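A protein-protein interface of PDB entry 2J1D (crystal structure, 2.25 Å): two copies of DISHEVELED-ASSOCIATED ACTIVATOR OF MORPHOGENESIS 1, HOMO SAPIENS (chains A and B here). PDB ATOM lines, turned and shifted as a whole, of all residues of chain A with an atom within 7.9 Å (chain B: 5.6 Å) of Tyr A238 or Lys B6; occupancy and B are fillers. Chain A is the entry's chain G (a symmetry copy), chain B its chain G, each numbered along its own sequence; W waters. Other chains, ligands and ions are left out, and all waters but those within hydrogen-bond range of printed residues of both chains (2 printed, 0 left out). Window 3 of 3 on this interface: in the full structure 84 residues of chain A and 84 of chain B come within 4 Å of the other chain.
The side-chain amide oxygen of Asn A227 lies close to the backbone carbonyl oxygen of Gly A235, at 3.3 Å. OD1 of Asn A227 sits at hydrogen-bond distance from N of Ala A237, 2.7 Å away. OD1 of Asn A227 sits close to N of Asn A236 (3.5 Å).
No position is printed for both chains. Of the 11 pairs that touch across the chains among the printed residues, none has its exchanged pair printed and touching as well.
Printed residues of chain B that touch a printed residue of chain A: Lys B6, Ile B8, Leu B23, Glu B25, Leu B28 and Trp B33. Hydrophobic or aromatic side chains of chain B that line the printed part of chain A: Ile B8, Leu B23, Leu B28 and Trp B33. Along chain A the printed residues that touch a printed residue of chain B span positions 219 to 240. Among the printed residues, 11 pairs touch across the chains.
Water W2 lies within hydrogen-bond range of N of Lys B6 (2.6 Å) and OH of Tyr A238 (3.5 Å). Water W1 bridges the backbone carbonyl oxygen (O) of Phe A240 (2.9 Å) and the indole nitrogen (NE1) of Trp B33 (3.0 Å).
Of the printed residues of chain B, Asn A227 touches Ile B8 (3.3 Å). Of chain B, only Lys B6, Glu B25, Leu B28 and Trp B33 come within 4 Å of Tyr A238. Of the printed residues of chain A, Leu B28 touches Tyr A238 (3.9 Å). Of the printed residues of chain A, Trp B33 touches Leu A219 (3.6 Å), Leu A223 (3.9 Å), Tyr A238 (3.5 Å), Gly A239 (3.6 Å) and Phe A240 (3.6 Å).
The backbone carbonyl oxygen of Gly A239 lies within hydrogen-bond range of the backbone NH of Leu B23, 2.9 Å away.
Among the printed residues, pairs that only touch across the chains: Asn A227 with Ile B8 (3.3 Å), Tyr A238 with Trp B33 (3.5 Å), Phe A240 with Leu B23 (3.5 Å), Leu A219 with Trp B33 (3.6 Å), Gly A239 with Trp B33 (3.6 Å), Phe A240 with Trp B33 (3.6 Å), Tyr A238 with Leu B28 (3.9 Å), Leu A223 with Trp B33 (3.9 Å), Tyr A238 with Lys B6 (3.98 Å) and Tyr A238 with Glu B25 (3.98 Å).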
ATOM      1  N   LEU A 219     -32.861 -34.863  15.001  1.00  0.00           N
ATOM      2  CA  LEU A 219     -31.930 -33.730  14.922  1.00  0.00           C
ATOM      3  C   LEU A 219     -31.982 -33.012  13.574  1.00  0.00           C
ATOM      4  O   LEU A 219     -31.893 -31.790  13.503  1.00  0.00           O
ATOM      5  CB  LEU A 219     -30.508 -34.224  15.168  1.00  0.00           C
ATOM      6  CG  LEU A 219     -30.202 -34.680  16.588  1.00  0.00           C
ATOM      7  CD1 LEU A 219     -28.791 -35.189  16.641  1.00  0.00           C
ATOM      8  CD2 LEU A 219     -30.403 -33.511  17.527  1.00  0.00           C
ATOM      9  N   LEU A 223     -33.289 -29.323  13.059  1.00  0.00           N
ATOM     10  CA  LEU A 223     -32.395 -28.391  12.372  1.00  0.00           C
ATOM     11  C   LEU A 223     -33.200 -27.626  11.326  1.00  0.00           C
ATOM     12  O   LEU A 223     -33.186 -26.404  11.283  1.00  0.00           O
ATOM     13  CB  LEU A 223     -31.230 -29.130  11.706  1.00  0.00           C
ATOM     14  CG  LEU A 223     -30.127 -28.261  11.098  1.00  0.00           C
ATOM     15  CD1 LEU A 223     -29.524 -27.283  12.111  1.00  0.00           C
ATOM     16  CD2 LEU A 223     -29.059 -29.145  10.510  1.00  0.00           C
ATOM     17  N   ASN A 227     -33.796 -23.552  11.137  1.00  0.00           N
ATOM     18  CA  ASN A 227     -33.327 -22.868   9.926  1.00  0.00           C
ATOM     19  C   ASN A 227     -34.462 -22.160   9.151  1.00  0.00           C
ATOM     20  O   ASN A 227     -34.229 -21.158   8.481  1.00  0.00           O
ATOM     21  CB  ASN A 227     -32.561 -23.848   9.014  1.00  0.00           C
ATOM     22  CG  ASN A 227     -31.068 -23.947   9.360  1.00  0.00           C
ATOM     23  OD1 ASN A 227     -30.502 -23.055   9.986  1.00  0.00           O
ATOM     24  ND2 ASN A 227     -30.429 -25.031   8.934  1.00  0.00           N
ATOM     25  N   GLY A 235     -29.892 -18.478  11.464  1.00  0.00           N
ATOM     26  CA  GLY A 235     -30.538 -19.643  10.885  1.00  0.00           C
ATOM     27  C   GLY A 235     -30.024 -19.998   9.505  1.00  0.00           C
ATOM     28  O   GLY A 235     -30.805 -20.106   8.534  1.00  0.00           O
ATOM     29  N   ASN A 236     -28.701 -20.126   9.411  1.00  0.00           N
ATOM     30  CA  ASN A 236     -28.108 -21.046   8.449  1.00  0.00           C
ATOM     31  C   ASN A 236     -27.231 -22.031   9.203  1.00  0.00           C
ATOM     32  O   ASN A 236     -26.012 -22.061   9.022  1.00  0.00           O
ATOM     33  CB  ASN A 236     -27.292 -20.300   7.396  1.00  0.00           C
ATOM     34  CG  ASN A 236     -27.343 -20.979   6.032  1.00  0.00           C
ATOM     35  OD1 ASN A 236     -28.057 -21.966   5.828  1.00  0.00           O
ATOM     36  ND2 ASN A 236     -26.592 -20.433   5.080  1.00  0.00           N
ATOM     37  N   ALA A 237     -27.855 -22.826  10.064  1.00  0.00           N
ATOM     38  CA  ALA A 237     -27.119 -23.760  10.903  1.00  0.00           C
ATOM     39  C   ALA A 237     -26.828 -25.056  10.153  1.00  0.00           C
ATOM     40  O   ALA A 237     -27.612 -25.485   9.303  1.00  0.00           O
ATOM     41  CB  ALA A 237     -27.897 -24.044  12.175  1.00  0.00           C
ATOM     42  N   TYR A 238     -25.679 -25.652  10.451  1.00  0.00           N
ATOM     43  CA  TYR A 238     -25.373 -27.026  10.031  1.00  0.00           C
ATOM     44  C   TYR A 238     -25.453 -28.010  11.200  1.00  0.00           C
ATOM     45  O   TYR A 238     -25.368 -29.225  11.009  1.00  0.00           O
ATOM     46  CB  TYR A 238     -24.003 -27.076   9.353  1.00  0.00           C
ATOM     47  CG  TYR A 238     -24.049 -26.355   8.043  1.00  0.00           C
ATOM     48  CD1 TYR A 238     -24.466 -27.009   6.892  1.00  0.00           C
ATOM     49  CD2 TYR A 238     -23.747 -24.995   7.961  1.00  0.00           C
ATOM     50  CE1 TYR A 238     -24.552 -26.339   5.678  1.00  0.00           C
ATOM     51  CE2 TYR A 238     -23.823 -24.314   6.750  1.00  0.00           C
ATOM     52  CZ  TYR A 238     -24.228 -24.993   5.613  1.00  0.00           C
ATOM     53  OH  TYR A 238     -24.308 -24.336   4.407  1.00  0.00           O
ATOM     54  N   GLY A 239     -25.645 -27.465  12.399  1.00  0.00           N
ATOM     55  CA  GLY A 239     -25.755 -28.239  13.618  1.00  0.00           C
ATOM     56  C   GLY A 239     -26.021 -27.342  14.804  1.00  0.00           C
ATOM     57  O   GLY A 239     -25.800 -26.149  14.731  1.00  0.00           O
ATOM     58  N   PHE A 240     -26.505 -27.915  15.897  1.00  0.00           N
ATOM     59  CA  PHE A 240     -26.721 -27.164  17.131  1.00  0.00           C
ATOM     60  C   PHE A 240     -26.231 -27.959  18.337  1.00  0.00           C
ATOM     61  O   PHE A 240     -25.987 -29.160  18.232  1.00  0.00           O
ATOM     62  CB  PHE A 240     -28.198 -26.762  17.285  1.00  0.00           C
ATOM     63  CG  PHE A 240     -29.180 -27.910  17.171  1.00  0.00           C
ATOM     64  CD1 PHE A 240     -29.398 -28.770  18.236  1.00  0.00           C
ATOM     65  CD2 PHE A 240     -29.924 -28.094  16.011  1.00  0.00           C
ATOM     66  CE1 PHE A 240     -30.322 -29.821  18.134  1.00  0.00           C
ATOM     67  CE2 PHE A 240     -30.849 -29.128  15.903  1.00  0.00           C
ATOM     68  CZ  PHE A 240     -31.047 -29.990  16.964  1.00  0.00           C
ATOM     69  N   LYS B   6     -25.866 -23.952  -0.025  1.00  0.00           N
ATOM     70  CA  LYS B   6     -26.548 -23.508   1.229  1.00  0.00           C
ATOM     71  C   LYS B   6     -27.984 -24.077   1.291  1.00  0.00           C
ATOM     72  O   LYS B   6     -28.273 -24.943   2.118  1.00  0.00           O
ATOM     73  CB  LYS B   6     -26.536 -21.973   1.317  1.00  0.00           C
ATOM     74  CG  LYS B   6     -25.134 -21.355   1.357  1.00  0.00           C
ATOM     75  CD  LYS B   6     -25.178 -19.849   1.116  1.00  0.00           C
ATOM     76  CE  LYS B   6     -23.792 -19.270   0.825  1.00  0.00           C
ATOM     77  NZ  LYS B   6     -23.862 -17.941   0.149  1.00  0.00           N
ATOM     78  N   SER B   7     -28.858 -23.573   0.412  1.00  0.00           N
ATOM     79  CA  SER B   7     -30.203 -24.210   0.031  1.00  0.00           C
ATOM     80  C   SER B   7     -31.559 -24.252   0.729  1.00  0.00           C
ATOM     81  O   SER B   7     -32.456 -24.921   0.194  1.00  0.00           O
ATOM     82  CB  SER B   7     -30.009 -25.727  -0.166  1.00  0.00           C
ATOM     83  OG  SER B   7     -31.156 -26.307  -0.817  1.00  0.00           O
ATOM     84  N   ILE B   8     -31.927 -23.610   1.866  1.00  0.00           N
ATOM     85  CA  ILE B   8     -33.184 -23.887   2.531  1.00  0.00           C
ATOM     86  C   ILE B   8     -34.179 -22.801   2.045  1.00  0.00           C
ATOM     87  O   ILE B   8     -33.742 -21.701   1.687  1.00  0.00           O
ATOM     88  CB  ILE B   8     -32.898 -23.875   4.056  1.00  0.00           C
ATOM     89  CG1 ILE B   8     -32.702 -22.445   4.556  1.00  0.00           C
ATOM     90  CG2 ILE B   8     -31.651 -24.720   4.367  1.00  0.00           C
ATOM     91  CD1 ILE B   8     -33.938 -21.862   5.220  1.00  0.00           C
ATOM     92  N   LEU B  23     -23.943 -25.045  16.714  1.00  0.00           N
ATOM     93  CA  LEU B  23     -22.578 -25.539  16.760  1.00  0.00           C
ATOM     94  C   LEU B  23     -21.768 -24.787  15.713  1.00  0.00           C
ATOM     95  O   LEU B  23     -22.176 -24.722  14.552  1.00  0.00           O
ATOM     96  CB  LEU B  23     -22.505 -27.029  16.422  1.00  0.00           C
ATOM     97  CG  LEU B  23     -22.512 -28.109  17.498  1.00  0.00           C
ATOM     98  CD1 LEU B  23     -21.959 -29.372  16.857  1.00  0.00           C
ATOM     99  CD2 LEU B  23     -21.714 -27.741  18.722  1.00  0.00           C
ATOM    100  N   GLU B  25     -19.178 -24.337  12.807  1.00  0.00           N
ATOM    101  CA  GLU B  25     -18.859 -25.281  11.737  1.00  0.00           C
ATOM    102  C   GLU B  25     -17.460 -25.894  11.923  1.00  0.00           C
ATOM    103  O   GLU B  25     -17.198 -27.013  11.469  1.00  0.00           O
ATOM    104  CB  GLU B  25     -18.987 -24.606  10.366  1.00  0.00           C
ATOM    105  CG  GLU B  25     -20.425 -24.177   9.993  1.00  0.00           C
ATOM    106  CD  GLU B  25     -20.715 -22.695  10.234  1.00  0.00           C
ATOM    107  OE1 GLU B  25     -21.803 -22.376  10.772  1.00  0.00           O
ATOM    108  OE2 GLU B  25     -19.863 -21.850   9.875  1.00  0.00           O
ATOM    109  N   LEU B  28     -17.473 -29.452  13.551  1.00  0.00           N
ATOM    110  CA  LEU B  28     -18.058 -30.608  12.876  1.00  0.00           C
ATOM    111  C   LEU B  28     -16.947 -31.512  12.364  1.00  0.00           C
ATOM    112  O   LEU B  28     -15.828 -31.466  12.877  1.00  0.00           O
ATOM    113  CB  LEU B  28     -18.961 -30.162  11.727  1.00  0.00           C
ATOM    114  CG  LEU B  28     -19.994 -29.075  12.056  1.00  0.00           C
ATOM    115  CD1 LEU B  28     -20.887 -28.810  10.863  1.00  0.00           C
ATOM    116  CD2 LEU B  28     -20.846 -29.424  13.266  1.00  0.00           C
ATOM    117  N   TRP B  33     -23.566 -34.599  12.386  1.00  0.00           N
ATOM    118  CA  TRP B  33     -24.066 -33.600  11.445  1.00  0.00           C
ATOM    119  C   TRP B  33     -23.503 -33.786  10.035  1.00  0.00           C
ATOM    120  O   TRP B  33     -24.163 -33.470   9.056  1.00  0.00           O
ATOM    121  CB  TRP B  33     -23.803 -32.211  11.999  1.00  0.00           C
ATOM    122  CG  TRP B  33     -24.423 -32.041  13.352  1.00  0.00           C
ATOM    123  CD1 TRP B  33     -23.781 -32.076  14.550  1.00  0.00           C
ATOM    124  CD2 TRP B  33     -25.811 -31.858  13.645  1.00  0.00           C
ATOM    125  NE1 TRP B  33     -24.677 -31.905  15.573  1.00  0.00           N
ATOM    126  CE2 TRP B  33     -25.932 -31.768  15.045  1.00  0.00           C
ATOM    127  CE3 TRP B  33     -26.964 -31.747  12.860  1.00  0.00           C
ATOM    128  CZ2 TRP B  33     -27.161 -31.584  15.680  1.00  0.00           C
ATOM    129  CZ3 TRP B  33     -28.183 -31.545  13.494  1.00  0.00           C
ATOM    130  CH2 TRP B  33     -28.268 -31.459  14.889  1.00  0.00           C
ATOM    131  N   THR B  39     -32.058 -30.273   4.156  1.00  0.00           N
ATOM    132  CA  THR B  39     -32.640 -29.785   2.896  1.00  0.00           C
ATOM    133  C   THR B  39     -33.708 -30.718   2.311  1.00  0.00           C
ATOM    134  O   THR B  39     -34.544 -30.280   1.524  1.00  0.00           O
ATOM    135  CB  THR B  39     -31.569 -29.475   1.825  1.00  0.00           C
ATOM    136  OG1 THR B  39     -30.845 -30.666   1.508  1.00  0.00           O
ATOM    137  CG2 THR B  39     -30.608 -28.411   2.331  1.00  0.00           C
HETATM  138  O   HOH W   1     -24.921 -31.784  18.566  1.00  0.00           O
HETATM  139  O   HOH W   2     -23.871 -25.250   1.074  1.00  0.00           O
